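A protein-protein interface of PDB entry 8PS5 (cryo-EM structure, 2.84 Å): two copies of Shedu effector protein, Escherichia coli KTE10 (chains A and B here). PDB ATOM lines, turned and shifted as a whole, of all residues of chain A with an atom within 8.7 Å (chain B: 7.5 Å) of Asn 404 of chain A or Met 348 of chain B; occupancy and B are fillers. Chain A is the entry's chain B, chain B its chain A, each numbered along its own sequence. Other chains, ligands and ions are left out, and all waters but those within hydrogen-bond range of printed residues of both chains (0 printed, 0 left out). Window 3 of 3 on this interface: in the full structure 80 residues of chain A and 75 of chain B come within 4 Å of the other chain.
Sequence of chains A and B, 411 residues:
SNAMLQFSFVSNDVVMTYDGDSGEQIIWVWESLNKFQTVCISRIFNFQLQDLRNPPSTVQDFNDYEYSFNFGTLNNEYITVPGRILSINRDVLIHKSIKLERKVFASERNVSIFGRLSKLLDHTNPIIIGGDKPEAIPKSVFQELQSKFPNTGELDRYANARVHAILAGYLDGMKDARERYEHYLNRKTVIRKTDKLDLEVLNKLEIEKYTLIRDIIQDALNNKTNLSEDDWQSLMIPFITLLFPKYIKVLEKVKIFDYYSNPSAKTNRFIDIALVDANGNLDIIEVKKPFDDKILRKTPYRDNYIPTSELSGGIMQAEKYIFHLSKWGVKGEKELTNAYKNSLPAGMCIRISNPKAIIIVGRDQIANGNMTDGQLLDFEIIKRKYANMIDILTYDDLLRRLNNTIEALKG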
ATOM      1  N   TYR A 210     -17.637 -23.362 -16.043  1.00  0.00           N
ATOM      2  CA  TYR A 210     -16.390 -22.606 -16.016  1.00  0.00           C
ATOM      3  C   TYR A 210     -15.645 -22.692 -17.346  1.00  0.00           C
ATOM      4  O   TYR A 210     -14.982 -21.723 -17.740  1.00  0.00           O
ATOM      5  CB  TYR A 210     -15.518 -23.077 -14.854  1.00  0.00           C
ATOM      6  CG  TYR A 210     -15.948 -22.499 -13.521  1.00  0.00           C
ATOM      7  CD1 TYR A 210     -16.416 -21.190 -13.433  1.00  0.00           C
ATOM      8  CD2 TYR A 210     -15.886 -23.259 -12.356  1.00  0.00           C
ATOM      9  CE1 TYR A 210     -16.815 -20.652 -12.219  1.00  0.00           C
ATOM     10  CE2 TYR A 210     -16.284 -22.730 -11.135  1.00  0.00           C
ATOM     11  CZ  TYR A 210     -16.746 -21.426 -11.077  1.00  0.00           C
ATOM     12  OH  TYR A 210     -17.139 -20.889  -9.874  1.00  0.00           O
ATOM     13  N   ARG A 214     -14.805 -19.389 -19.505  1.00  0.00           N
ATOM     14  CA  ARG A 214     -13.420 -19.241 -19.953  1.00  0.00           C
ATOM     15  C   ARG A 214     -13.315 -19.136 -21.472  1.00  0.00           C
ATOM     16  O   ARG A 214     -12.569 -18.295 -21.988  1.00  0.00           O
ATOM     17  CB  ARG A 214     -12.587 -20.417 -19.444  1.00  0.00           C
ATOM     18  CG  ARG A 214     -11.093 -20.247 -19.616  1.00  0.00           C
ATOM     19  CD  ARG A 214     -10.395 -21.578 -19.799  1.00  0.00           C
ATOM     20  NE  ARG A 214     -11.034 -22.390 -20.825  1.00  0.00           N
ATOM     21  CZ  ARG A 214     -10.965 -23.712 -20.882  1.00  0.00           C
ATOM     22  NH1 ARG A 214     -10.294 -24.408 -19.980  1.00  0.00           N
ATOM     23  NH2 ARG A 214     -11.584 -24.351 -21.869  1.00  0.00           N
ATOM     24  N   ASP A 396      -5.700 -12.368 -18.380  1.00  0.00           N
ATOM     25  CA  ASP A 396      -4.986 -13.637 -18.343  1.00  0.00           C
ATOM     26  C   ASP A 396      -4.958 -14.220 -16.934  1.00  0.00           C
ATOM     27  O   ASP A 396      -4.900 -15.442 -16.775  1.00  0.00           O
ATOM     28  CB  ASP A 396      -3.573 -13.462 -18.889  1.00  0.00           C
ATOM     29  CG  ASP A 396      -3.549 -12.763 -20.233  1.00  0.00           C
ATOM     30  OD1 ASP A 396      -4.621 -12.644 -20.863  1.00  0.00           O
ATOM     31  OD2 ASP A 396      -2.459 -12.336 -20.664  1.00  0.00           O
ATOM     32  N   ASP A 397      -5.025 -13.369 -15.900  1.00  0.00           N
ATOM     33  CA  ASP A 397      -5.192 -13.882 -14.538  1.00  0.00           C
ATOM     34  C   ASP A 397      -6.580 -14.469 -14.345  1.00  0.00           C
ATOM     35  O   ASP A 397      -6.744 -15.448 -13.613  1.00  0.00           O
ATOM     36  CB  ASP A 397      -4.957 -12.792 -13.493  1.00  0.00           C
ATOM     37  CG  ASP A 397      -3.492 -12.605 -13.160  1.00  0.00           C
ATOM     38  OD1 ASP A 397      -2.650 -13.323 -13.736  1.00  0.00           O
ATOM     39  OD2 ASP A 397      -3.183 -11.735 -12.321  1.00  0.00           O
ATOM     40  N   LEU A 398      -7.585 -13.875 -14.996  1.00  0.00           N
ATOM     41  CA  LEU A 398      -8.941 -14.419 -14.970  1.00  0.00           C
ATOM     42  C   LEU A 398      -9.011 -15.769 -15.672  1.00  0.00           C
ATOM     43  O   LEU A 398      -9.636 -16.706 -15.161  1.00  0.00           O
ATOM     44  CB  LEU A 398      -9.905 -13.425 -15.613  1.00  0.00           C
ATOM     45  CG  LEU A 398     -11.393 -13.559 -15.297  1.00  0.00           C
ATOM     46  CD1 LEU A 398     -11.628 -13.477 -13.802  1.00  0.00           C
ATOM     47  CD2 LEU A 398     -12.173 -12.480 -16.022  1.00  0.00           C
ATOM     48  N   LEU A 399      -8.331 -15.897 -16.818  1.00  0.00           N
ATOM     49  CA  LEU A 399      -8.287 -17.176 -17.528  1.00  0.00           C
ATOM     50  C   LEU A 399      -7.470 -18.217 -16.767  1.00  0.00           C
ATOM     51  O   LEU A 399      -7.819 -19.404 -16.762  1.00  0.00           O
ATOM     52  CB  LEU A 399      -7.718 -16.975 -18.932  1.00  0.00           C
ATOM     53  CG  LEU A 399      -8.546 -16.151 -19.919  1.00  0.00           C
ATOM     54  CD1 LEU A 399      -7.845 -16.073 -21.259  1.00  0.00           C
ATOM     55  CD2 LEU A 399      -9.937 -16.716 -20.076  1.00  0.00           C
ATOM     56  N   ARG A 400      -6.398 -17.784 -16.092  1.00  0.00           N
ATOM     57  CA  ARG A 400      -5.575 -18.688 -15.294  1.00  0.00           C
ATOM     58  C   ARG A 400      -6.318 -19.179 -14.058  1.00  0.00           C
ATOM     59  O   ARG A 400      -6.215 -20.354 -13.688  1.00  0.00           O
ATOM     60  CB  ARG A 400      -4.283 -17.981 -14.888  1.00  0.00           C
ATOM     61  CG  ARG A 400      -3.050 -18.856 -14.900  1.00  0.00           C
ATOM     62  CD  ARG A 400      -1.793 -18.013 -14.782  1.00  0.00           C
ATOM     63  NE  ARG A 400      -1.728 -16.971 -15.798  1.00  0.00           N
ATOM     64  CZ  ARG A 400      -1.460 -15.697 -15.546  1.00  0.00           C
ATOM     65  NH1 ARG A 400      -1.249 -15.267 -14.314  1.00  0.00           N
ATOM     66  NH2 ARG A 400      -1.405 -14.833 -16.556  1.00  0.00           N
ATOM     67  N   ARG A 401      -7.091 -18.295 -13.421  1.00  0.00           N
ATOM     68  CA  ARG A 401      -7.877 -18.688 -12.259  1.00  0.00           C
ATOM     69  C   ARG A 401      -9.050 -19.572 -12.658  1.00  0.00           C
ATOM     70  O   ARG A 401      -9.422 -20.487 -11.914  1.00  0.00           O
ATOM     71  CB  ARG A 401      -8.362 -17.447 -11.515  1.00  0.00           C
ATOM     72  CG  ARG A 401      -7.302 -16.822 -10.629  1.00  0.00           C
ATOM     73  CD  ARG A 401      -7.613 -15.378 -10.338  1.00  0.00           C
ATOM     74  NE  ARG A 401      -8.945 -15.213  -9.773  1.00  0.00           N
ATOM     75  CZ  ARG A 401      -9.225 -14.434  -8.738  1.00  0.00           C
ATOM     76  NH1 ARG A 401      -8.288 -13.719  -8.137  1.00  0.00           N
ATOM     77  NH2 ARG A 401     -10.478 -14.368  -8.297  1.00  0.00           N
ATOM     78  N   LEU A 402      -9.628 -19.327 -13.845  1.00  0.00           N
ATOM     79  CA  LEU A 402     -10.671 -20.206 -14.371  1.00  0.00           C
ATOM     80  C   LEU A 402     -10.124 -21.592 -14.686  1.00  0.00           C
ATOM     81  O   LEU A 402     -10.765 -22.601 -14.368  1.00  0.00           O
ATOM     82  CB  LEU A 402     -11.308 -19.587 -15.614  1.00  0.00           C
ATOM     83  CG  LEU A 402     -12.435 -18.583 -15.371  1.00  0.00           C
ATOM     84  CD1 LEU A 402     -12.575 -17.639 -16.552  1.00  0.00           C
ATOM     85  CD2 LEU A 402     -13.739 -19.298 -15.102  1.00  0.00           C
ATOM     86  N   ASN A 403      -8.914 -21.658 -15.259  1.00  0.00           N
ATOM     87  CA  ASN A 403      -8.268 -22.938 -15.538  1.00  0.00           C
ATOM     88  C   ASN A 403      -7.879 -23.667 -14.254  1.00  0.00           C
ATOM     89  O   ASN A 403      -7.931 -24.901 -14.195  1.00  0.00           O
ATOM     90  CB  ASN A 403      -7.039 -22.717 -16.417  1.00  0.00           C
ATOM     91  CG  ASN A 403      -7.390 -22.581 -17.882  1.00  0.00           C
ATOM     92  OD1 ASN A 403      -7.912 -23.511 -18.496  1.00  0.00           O
ATOM     93  ND2 ASN A 403      -7.105 -21.418 -18.454  1.00  0.00           N
ATOM     94  N   ASN A 404      -7.516 -22.916 -13.208  1.00  0.00           N
ATOM     95  CA  ASN A 404      -7.214 -23.533 -11.919  1.00  0.00           C
ATOM     96  C   ASN A 404      -8.469 -24.076 -11.240  1.00  0.00           C
ATOM     97  O   ASN A 404      -8.415 -25.135 -10.606  1.00  0.00           O
ATOM     98  CB  ASN A 404      -6.498 -22.538 -11.008  1.00  0.00           C
ATOM     99  CG  ASN A 404      -5.052 -22.327 -11.403  1.00  0.00           C
ATOM    100  OD1 ASN A 404      -4.383 -23.251 -11.859  1.00  0.00           O
ATOM    101  ND2 ASN A 404      -4.561 -21.109 -11.221  1.00  0.00           N
ATOM    102  N   THR A 405      -9.607 -23.377 -11.376  1.00  0.00           N
ATOM    103  CA  THR A 405     -10.871 -23.907 -10.855  1.00  0.00           C
ATOM    104  C   THR A 405     -11.322 -25.145 -11.622  1.00  0.00           C
ATOM    105  O   THR A 405     -11.859 -26.083 -11.023  1.00  0.00           O
ATOM    106  CB  THR A 405     -11.984 -22.857 -10.899  1.00  0.00           C
ATOM    107  OG1 THR A 405     -12.096 -22.327 -12.222  1.00  0.00           O
ATOM    108  CG2 THR A 405     -11.742 -21.738  -9.908  1.00  0.00           C
ATOM    109  N   ILE A 406     -11.099 -25.163 -12.944  1.00  0.00           N
ATOM    110  CA  ILE A 406     -11.436 -26.326 -13.770  1.00  0.00           C
ATOM    111  C   ILE A 406     -10.571 -27.531 -13.397  1.00  0.00           C
ATOM    112  O   ILE A 406     -11.082 -28.643 -13.201  1.00  0.00           O
ATOM    113  CB  ILE A 406     -11.312 -25.963 -15.266  1.00  0.00           C
ATOM    114  CG1 ILE A 406     -12.490 -25.099 -15.708  1.00  0.00           C
ATOM    115  CG2 ILE A 406     -11.247 -27.194 -16.158  1.00  0.00           C
ATOM    116  CD1 ILE A 406     -12.176 -24.211 -16.889  1.00  0.00           C
ATOM    117  N   GLU A 407      -9.262 -27.315 -13.224  1.00  0.00           N
ATOM    118  CA  GLU A 407      -8.367 -28.419 -12.889  1.00  0.00           C
ATOM    119  C   GLU A 407      -8.523 -28.857 -11.434  1.00  0.00           C
ATOM    120  O   GLU A 407      -8.196 -29.998 -11.087  1.00  0.00           O
ATOM    121  CB  GLU A 407      -6.919 -28.025 -13.180  1.00  0.00           C
ATOM    122  CG  GLU A 407      -6.063 -29.156 -13.736  1.00  0.00           C
ATOM    123  CD  GLU A 407      -6.564 -29.689 -15.072  1.00  0.00           C
ATOM    124  OE1 GLU A 407      -6.490 -30.917 -15.286  1.00  0.00           O
ATOM    125  OE2 GLU A 407      -7.006 -28.882 -15.918  1.00  0.00           O
ATOM    126  N   ALA A 408      -9.019 -27.970 -10.568  1.00  0.00           N
ATOM    127  CA  ALA A 408      -9.315 -28.368  -9.196  1.00  0.00           C
ATOM    128  C   ALA A 408     -10.617 -29.157  -9.120  1.00  0.00           C
ATOM    129  O   ALA A 408     -10.735 -30.104  -8.336  1.00  0.00           O
ATOM    130  CB  ALA A 408      -9.379 -27.137  -8.296  1.00  0.00           C
ATOM    131  N   LEU A 409     -11.614 -28.770  -9.922  1.00  0.00           N
ATOM    132  CA  LEU A 409     -12.888 -29.481  -9.912  1.00  0.00           C
ATOM    133  C   LEU A 409     -12.789 -30.817 -10.639  1.00  0.00           C
ATOM    134  O   LEU A 409     -13.590 -31.726 -10.389  1.00  0.00           O
ATOM    135  CB  LEU A 409     -13.979 -28.612 -10.537  1.00  0.00           C
ATOM    136  CG  LEU A 409     -14.636 -27.534  -9.678  1.00  0.00           C
ATOM    137  CD1 LEU A 409     -15.181 -26.427 -10.556  1.00  0.00           C
ATOM    138  CD2 LEU A 409     -15.741 -28.132  -8.832  1.00  0.00           C
ATOM    139  N   LYS A 410     -11.828 -30.947 -11.560  1.00  0.00           N
ATOM    140  CA  LYS A 410     -11.614 -32.227 -12.229  1.00  0.00           C
ATOM    141  C   LYS A 410     -10.994 -33.251 -11.287  1.00  0.00           C
ATOM    142  O   LYS A 410     -11.339 -34.437 -11.331  1.00  0.00           O
ATOM    143  CB  LYS A 410     -10.734 -32.037 -13.464  1.00  0.00           C
ATOM    144  CG  LYS A 410     -11.493 -31.609 -14.705  1.00  0.00           C
ATOM    145  CD  LYS A 410     -10.715 -31.933 -15.966  1.00  0.00           C
ATOM    146  CE  LYS A 410     -10.994 -30.920 -17.060  1.00  0.00           C
ATOM    147  NZ  LYS A 410      -9.781 -30.125 -17.394  1.00  0.00           N
ATOM    148  N   GLY A 411     -10.081 -32.813 -10.427  1.00  0.00           N
ATOM    149  CA  GLY A 411      -9.450 -33.701  -9.468  1.00  0.00           C
ATOM    150  C   GLY A 411      -8.370 -34.576 -10.073  1.00  0.00           C
ATOM    151  O   GLY A 411      -7.592 -35.203  -9.355  1.00  0.00           O
ATOM    152  N   ILE B 248     -10.548 -23.090  -4.116  1.00  0.00           N
ATOM    153  CA  ILE B 248     -10.629 -24.201  -5.057  1.00  0.00           C
ATOM    154  C   ILE B 248     -10.241 -25.546  -4.445  1.00  0.00           C
ATOM    155  O   ILE B 248     -10.489 -26.588  -5.071  1.00  0.00           O
ATOM    156  CB  ILE B 248      -9.767 -23.919  -6.308  1.00  0.00           C
ATOM    157  CG1 ILE B 248      -8.291 -24.246  -6.058  1.00  0.00           C
ATOM    158  CG2 ILE B 248      -9.906 -22.475  -6.728  1.00  0.00           C
ATOM    159  CD1 ILE B 248      -7.404 -24.022  -7.256  1.00  0.00           C
ATOM    160  N   LYS B 249      -9.655 -25.559  -3.252  1.00  0.00           N
ATOM    161  CA  LYS B 249      -9.153 -26.785  -2.655  1.00  0.00           C
ATOM    162  C   LYS B 249      -9.379 -26.753  -1.153  1.00  0.00           C
ATOM    163  O   LYS B 249      -9.086 -25.754  -0.492  1.00  0.00           O
ATOM    164  CB  LYS B 249      -7.663 -26.981  -2.966  1.00  0.00           C
ATOM    165  CG  LYS B 249      -7.088 -28.305  -2.496  1.00  0.00           C
ATOM    166  CD  LYS B 249      -7.831 -29.473  -3.119  1.00  0.00           C
ATOM    167  CE  LYS B 249      -7.247 -30.798  -2.671  1.00  0.00           C
ATOM    168  NZ  LYS B 249      -8.089 -31.947  -3.099  1.00  0.00           N
ATOM    169  N   VAL B 276      -7.485 -23.151  -0.068  1.00  0.00           N
ATOM    170  CA  VAL B 276      -6.492 -22.656  -1.016  1.00  0.00           C
ATOM    171  C   VAL B 276      -7.215 -21.861  -2.095  1.00  0.00           C
ATOM    172  O   VAL B 276      -8.207 -22.334  -2.661  1.00  0.00           O
ATOM    173  CB  VAL B 276      -5.683 -23.811  -1.634  1.00  0.00           C
ATOM    174  CG1 VAL B 276      -4.565 -23.286  -2.523  1.00  0.00           C
ATOM    175  CG2 VAL B 276      -5.119 -24.703  -0.557  1.00  0.00           C
ATOM    176  N   ASP B 277      -6.718 -20.658  -2.380  1.00  0.00           N
ATOM    177  CA  ASP B 277      -7.230 -19.825  -3.458  1.00  0.00           C
ATOM    178  C   ASP B 277      -6.856 -20.389  -4.826  1.00  0.00           C
ATOM    179  O   ASP B 277      -6.099 -21.353  -4.959  1.00  0.00           O
ATOM    180  CB  ASP B 277      -6.683 -18.402  -3.355  1.00  0.00           C
ATOM    181  CG  ASP B 277      -7.497 -17.529  -2.443  1.00  0.00           C
ATOM    182  OD1 ASP B 277      -8.612 -17.936  -2.083  1.00  0.00           O
ATOM    183  OD2 ASP B 277      -7.039 -16.420  -2.107  1.00  0.00           O
ATOM    184  N   ALA B 278      -7.385 -19.745  -5.867  1.00  0.00           N
ATOM    185  CA  ALA B 278      -6.951 -20.062  -7.221  1.00  0.00           C
ATOM    186  C   ALA B 278      -5.586 -19.451  -7.515  1.00  0.00           C
ATOM    187  O   ALA B 278      -4.876 -19.905  -8.419  1.00  0.00           O
ATOM    188  CB  ALA B 278      -7.991 -19.583  -8.230  1.00  0.00           C
ATOM    189  N   ASN B 279      -5.209 -18.407  -6.770  1.00  0.00           N
ATOM    190  CA  ASN B 279      -3.855 -17.872  -6.854  1.00  0.00           C
ATOM    191  C   ASN B 279      -2.867 -18.670  -6.018  1.00  0.00           C
ATOM    192  O   ASN B 279      -1.665 -18.609  -6.273  1.00  0.00           O
ATOM    193  CB  ASN B 279      -3.830 -16.413  -6.398  1.00  0.00           C
ATOM    194  CG  ASN B 279      -5.090 -15.663  -6.761  1.00  0.00           C
ATOM    195  OD1 ASN B 279      -5.299 -15.294  -7.915  1.00  0.00           O
ATOM    196  ND2 ASN B 279      -5.948 -15.441  -5.774  1.00  0.00           N
ATOM    197  N   GLY B 280      -3.338 -19.413  -5.027  1.00  0.00           N
ATOM    198  CA  GLY B 280      -2.471 -20.104  -4.099  1.00  0.00           C
ATOM    199  C   GLY B 280      -2.441 -19.548  -2.696  1.00  0.00           C
ATOM    200  O   GLY B 280      -1.649 -20.024  -1.882  1.00  0.00           O
ATOM    201  N   ASN B 281      -3.264 -18.556  -2.389  1.00  0.00           N
ATOM    202  CA  ASN B 281      -3.288 -18.017  -1.037  1.00  0.00           C
ATOM    203  C   ASN B 281      -4.045 -18.958  -0.107  1.00  0.00           C
ATOM    204  O   ASN B 281      -5.099 -19.490  -0.459  1.00  0.00           O
ATOM    205  CB  ASN B 281      -3.915 -16.622  -1.025  1.00  0.00           C
ATOM    206  CG  ASN B 281      -3.276 -15.687  -2.032  1.00  0.00           C
ATOM    207  OD1 ASN B 281      -2.052 -15.658  -2.182  1.00  0.00           O
ATOM    208  ND2 ASN B 281      -4.097 -14.903  -2.716  1.00  0.00           N
ATOM    209  N   THR B 337       3.915 -26.222   0.269  1.00  0.00           N
ATOM    210  CA  THR B 337       3.973 -26.595  -1.140  1.00  0.00           C
ATOM    211  C   THR B 337       4.554 -27.996  -1.314  1.00  0.00           C
ATOM    212  O   THR B 337       4.095 -28.762  -2.168  1.00  0.00           O
ATOM    213  CB  THR B 337       4.793 -25.554  -1.907  1.00  0.00           C
ATOM    214  OG1 THR B 337       4.293 -24.247  -1.605  1.00  0.00           O
ATOM    215  CG2 THR B 337       4.691 -25.762  -3.410  1.00  0.00           C
ATOM    216  N   TYR B 340       1.754 -30.451   0.027  1.00  0.00           N
ATOM    217  CA  TYR B 340       0.514 -30.507  -0.734  1.00  0.00           C
ATOM    218  C   TYR B 340       0.714 -30.241  -2.224  1.00  0.00           C
ATOM    219  O   TYR B 340      -0.074 -29.504  -2.821  1.00  0.00           O
ATOM    220  CB  TYR B 340      -0.497 -29.519  -0.153  1.00  0.00           C
ATOM    221  CG  TYR B 340      -0.972 -29.887   1.233  1.00  0.00           C
ATOM    222  CD1 TYR B 340      -1.802 -30.986   1.434  1.00  0.00           C
ATOM    223  CD2 TYR B 340      -0.581 -29.141   2.342  1.00  0.00           C
ATOM    224  CE1 TYR B 340      -2.238 -31.331   2.704  1.00  0.00           C
ATOM    225  CE2 TYR B 340      -1.009 -29.478   3.617  1.00  0.00           C
ATOM    226  CZ  TYR B 340      -1.837 -30.572   3.788  1.00  0.00           C
ATOM    227  OH  TYR B 340      -2.266 -30.912   5.049  1.00  0.00           O
ATOM    228  N   LYS B 341       1.750 -30.819  -2.835  1.00  0.00           N
ATOM    229  CA  LYS B 341       1.949 -30.627  -4.270  1.00  0.00           C
ATOM    230  C   LYS B 341       1.031 -31.530  -5.087  1.00  0.00           C
ATOM    231  O   LYS B 341       0.591 -31.152  -6.178  1.00  0.00           O
ATOM    232  CB  LYS B 341       3.414 -30.861  -4.647  1.00  0.00           C
ATOM    233  CG  LYS B 341       4.035 -32.137  -4.098  1.00  0.00           C
ATOM    234  CD  LYS B 341       5.548 -32.117  -4.243  1.00  0.00           C
ATOM    235  CE  LYS B 341       6.188 -33.290  -3.520  1.00  0.00           C
ATOM    236  NZ  LYS B 341       6.520 -34.404  -4.451  1.00  0.00           N
ATOM    237  N   LEU B 344      -2.784 -30.228  -5.053  1.00  0.00           N
ATOM    238  CA  LEU B 344      -3.013 -29.015  -5.816  1.00  0.00           C
ATOM    239  C   LEU B 344      -2.946 -29.307  -7.317  1.00  0.00           C
ATOM    240  O   LEU B 344      -2.403 -30.334  -7.732  1.00  0.00           O
ATOM    241  CB  LEU B 344      -1.970 -27.964  -5.435  1.00  0.00           C
ATOM    242  CG  LEU B 344      -2.186 -27.191  -4.132  1.00  0.00           C
ATOM    243  CD1 LEU B 344      -1.186 -26.057  -4.024  1.00  0.00           C
ATOM    244  CD2 LEU B 344      -3.606 -26.657  -4.046  1.00  0.00           C
ATOM    245  N   PRO B 345      -3.511 -28.430  -8.155  1.00  0.00           N
ATOM    246  CA  PRO B 345      -3.255 -28.524  -9.600  1.00  0.00           C
ATOM    247  C   PRO B 345      -1.816 -28.172  -9.962  1.00  0.00           C
ATOM    248  O   PRO B 345      -1.054 -27.648  -9.146  1.00  0.00           O
ATOM    249  CB  PRO B 345      -4.239 -27.515 -10.199  1.00  0.00           C
ATOM    250  CG  PRO B 345      -5.344 -27.455  -9.223  1.00  0.00           C
ATOM    251  CD  PRO B 345      -4.702 -27.602  -7.876  1.00  0.00           C
ATOM    252  N   ALA B 346      -1.450 -28.476 -11.209  1.00  0.00           N
ATOM    253  CA  ALA B 346      -0.086 -28.269 -11.683  1.00  0.00           C
ATOM    254  C   ALA B 346       0.231 -26.787 -11.849  1.00  0.00           C
ATOM    255  O   ALA B 346      -0.583 -26.012 -12.361  1.00  0.00           O
ATOM    256  CB  ALA B 346       0.126 -28.996 -13.009  1.00  0.00           C
ATOM    257  N   GLY B 347       1.424 -26.396 -11.407  1.00  0.00           N
ATOM    258  CA  GLY B 347       1.856 -25.015 -11.461  1.00  0.00           C
ATOM    259  C   GLY B 347       1.412 -24.161 -10.298  1.00  0.00           C
ATOM    260  O   GLY B 347       1.466 -22.930 -10.397  1.00  0.00           O
ATOM    261  N   MET B 348       0.968 -24.770  -9.205  1.00  0.00           N
ATOM    262  CA  MET B 348       0.361 -24.063  -8.088  1.00  0.00           C
ATOM    263  C   MET B 348       1.225 -24.242  -6.845  1.00  0.00           C
ATOM    264  O   MET B 348       1.709 -25.345  -6.574  1.00  0.00           O
ATOM    265  CB  MET B 348      -1.055 -24.590  -7.858  1.00  0.00           C
ATOM    266  CG  MET B 348      -2.119 -23.842  -8.630  1.00  0.00           C
ATOM    267  SD  MET B 348      -3.723 -23.912  -7.828  1.00  0.00           S
ATOM    268  CE  MET B 348      -3.437 -22.781  -6.492  1.00  0.00           C
ATOM    269  N   CYS B 349       1.438 -23.155  -6.112  1.00  0.00           N
ATOM    270  CA  CYS B 349       2.199 -23.178  -4.872  1.00  0.00           C
ATOM    271  C   CYS B 349       1.403 -22.480  -3.782  1.00  0.00           C
ATOM    272  O   CYS B 349       0.705 -21.498  -4.046  1.00  0.00           O
ATOM    273  CB  CYS B 349       3.563 -22.505  -5.041  1.00  0.00           C
ATOM    274  SG  CYS B 349       4.687 -23.348  -6.181  1.00  0.00           S
ATOM    275  N   ILE B 350       1.511 -22.989  -2.556  1.00  0.00           N
ATOM    276  CA  ILE B 350       0.790 -22.385  -1.443  1.00  0.00           C
ATOM    277  C   ILE B 350       1.565 -21.160  -0.979  1.00  0.00           C
ATOM    278  O   ILE B 350       2.754 -21.244  -0.649  1.00  0.00           O
ATOM    279  CB  ILE B 350       0.582 -23.405  -0.317  1.00  0.00           C
ATOM    280  CG1 ILE B 350      -0.550 -24.363  -0.679  1.00  0.00           C
ATOM    281  CG2 ILE B 350       0.227 -22.721   0.994  1.00  0.00           C
ATOM    282  CD1 ILE B 350      -0.564 -25.618   0.152  1.00  0.00           C
ATOM    283  N   ARG B 351       0.898 -20.008  -0.977  1.00  0.00           N
ATOM    284  CA  ARG B 351       1.485 -18.746  -0.549  1.00  0.00           C
ATOM    285  C   ARG B 351       0.752 -18.266   0.693  1.00  0.00           C
ATOM    286  O   ARG B 351      -0.480 -18.238   0.713  1.00  0.00           O
ATOM    287  CB  ARG B 351       1.401 -17.698  -1.660  1.00  0.00           C
ATOM    288  CG  ARG B 351       2.309 -17.969  -2.844  1.00  0.00           C
ATOM    289  CD  ARG B 351       1.541 -17.909  -4.151  1.00  0.00           C
ATOM    290  NE  ARG B 351       0.859 -16.633  -4.326  1.00  0.00           N
ATOM    291  CZ  ARG B 351       0.921 -15.894  -5.426  1.00  0.00           C
ATOM    292  NH1 ARG B 351       1.627 -16.278  -6.476  1.00  0.00           N
ATOM    293  NH2 ARG B 351       0.256 -14.744  -5.473  1.00  0.00           N
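OD1 of Asn 279 of chain B sits close to NH1 of Arg 401 of chain A, at 3.4 Å. The backbone carbonyl oxygen (O) of Ala 278 of chain B lies within hydrogen-bond range of the side-chain amide nitrogen (ND2) of Asn 404 of chain A (3.1 Å).
Of the 18 printed residues of chain A, 4 touch a printed residue of chain B. Hydrophobic or aromatic side chains of chain A within 4 Å of the printed part of chain B: Ala 408. Among the printed residues, no Asp or Glu carboxylate lies within 4 Å of a Lys or Arg side-chain nitrogen of the other chain.
Of the printed residues of chain B, Asn 404 of chain A touches Ile 248, Ala 278 and Met 348. Printed residues of chain A within 4 Å of Met 348 of chain B: Asn 404. No residue of chain A comes within 4 Å of Gly 347 of chain B. No residue of chain A comes within 4 Å of Cys 349 of chain B. Printed residues of chain A within 4 Å of Asn 279 of chain B: Arg 401. Of the printed residues of chain B, Arg 401 of chain A touches Ala 278 and Asn 279. Of the printed residues of chain A, Pro 345 of chain B touches Ala 408 (3.9 Å). Of the printed residues of chain B, Thr 405 of chain A touches Ile 248 (3.7 Å). The nearest printed residue of chain B that does not touch Asn 404 of chain A is Pro 345 of chain B (4.1 Å). The nearest printed residue of chain A that does not touch Met 348 of chain B is Ala 408 of chain A (6.5 Å). The nearest printed residue of chain A that does not touch Pro 345 of chain B is Glu 407 of chain A (4.04 Å).
Ala 278 of chain B touches Arg 401 of chain A (CB to CG, 3.7 Å). Ile 248 of chain B touches Asn 404 of chain A (CD1 to O, 3.7 Å). Met 348 of chain B touches Asn 404 of chain A. Ile 248 of chain B touches Thr 405 of chain A (CG2 to CG2, 3.7 Å). Ala 408 of chain A touches Ile 248 of chain B. Ala 408 of chain A touches Pro 345 of chain B (N to CG, 3.9 Å).
The backbone carbonyl oxygen (O) of Arg 401 of chain A lies within hydrogen-bond range of the side-chain hydroxyl (OG1) of Thr 405 of chain A. O of Leu 402 of chain A lies within hydrogen-bond range of OG1 of Thr 405 of chain A (2.5 Å). O of Val 276 of chain B lies within hydrogen-bond range of N of Ile 248 of chain B, at 2.9 Å. The backbone carbonyl oxygen (O) of Arg 400 of chain A lies within hydrogen-bond range of the side-chain amide nitrogen (ND2) of Asn 404 of chain A, 3.1 Å away.
No position is printed for both chains. Of the 8 pairs that touch across the chains among the printed residues, none has its exchanged pair printed and touching as well.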
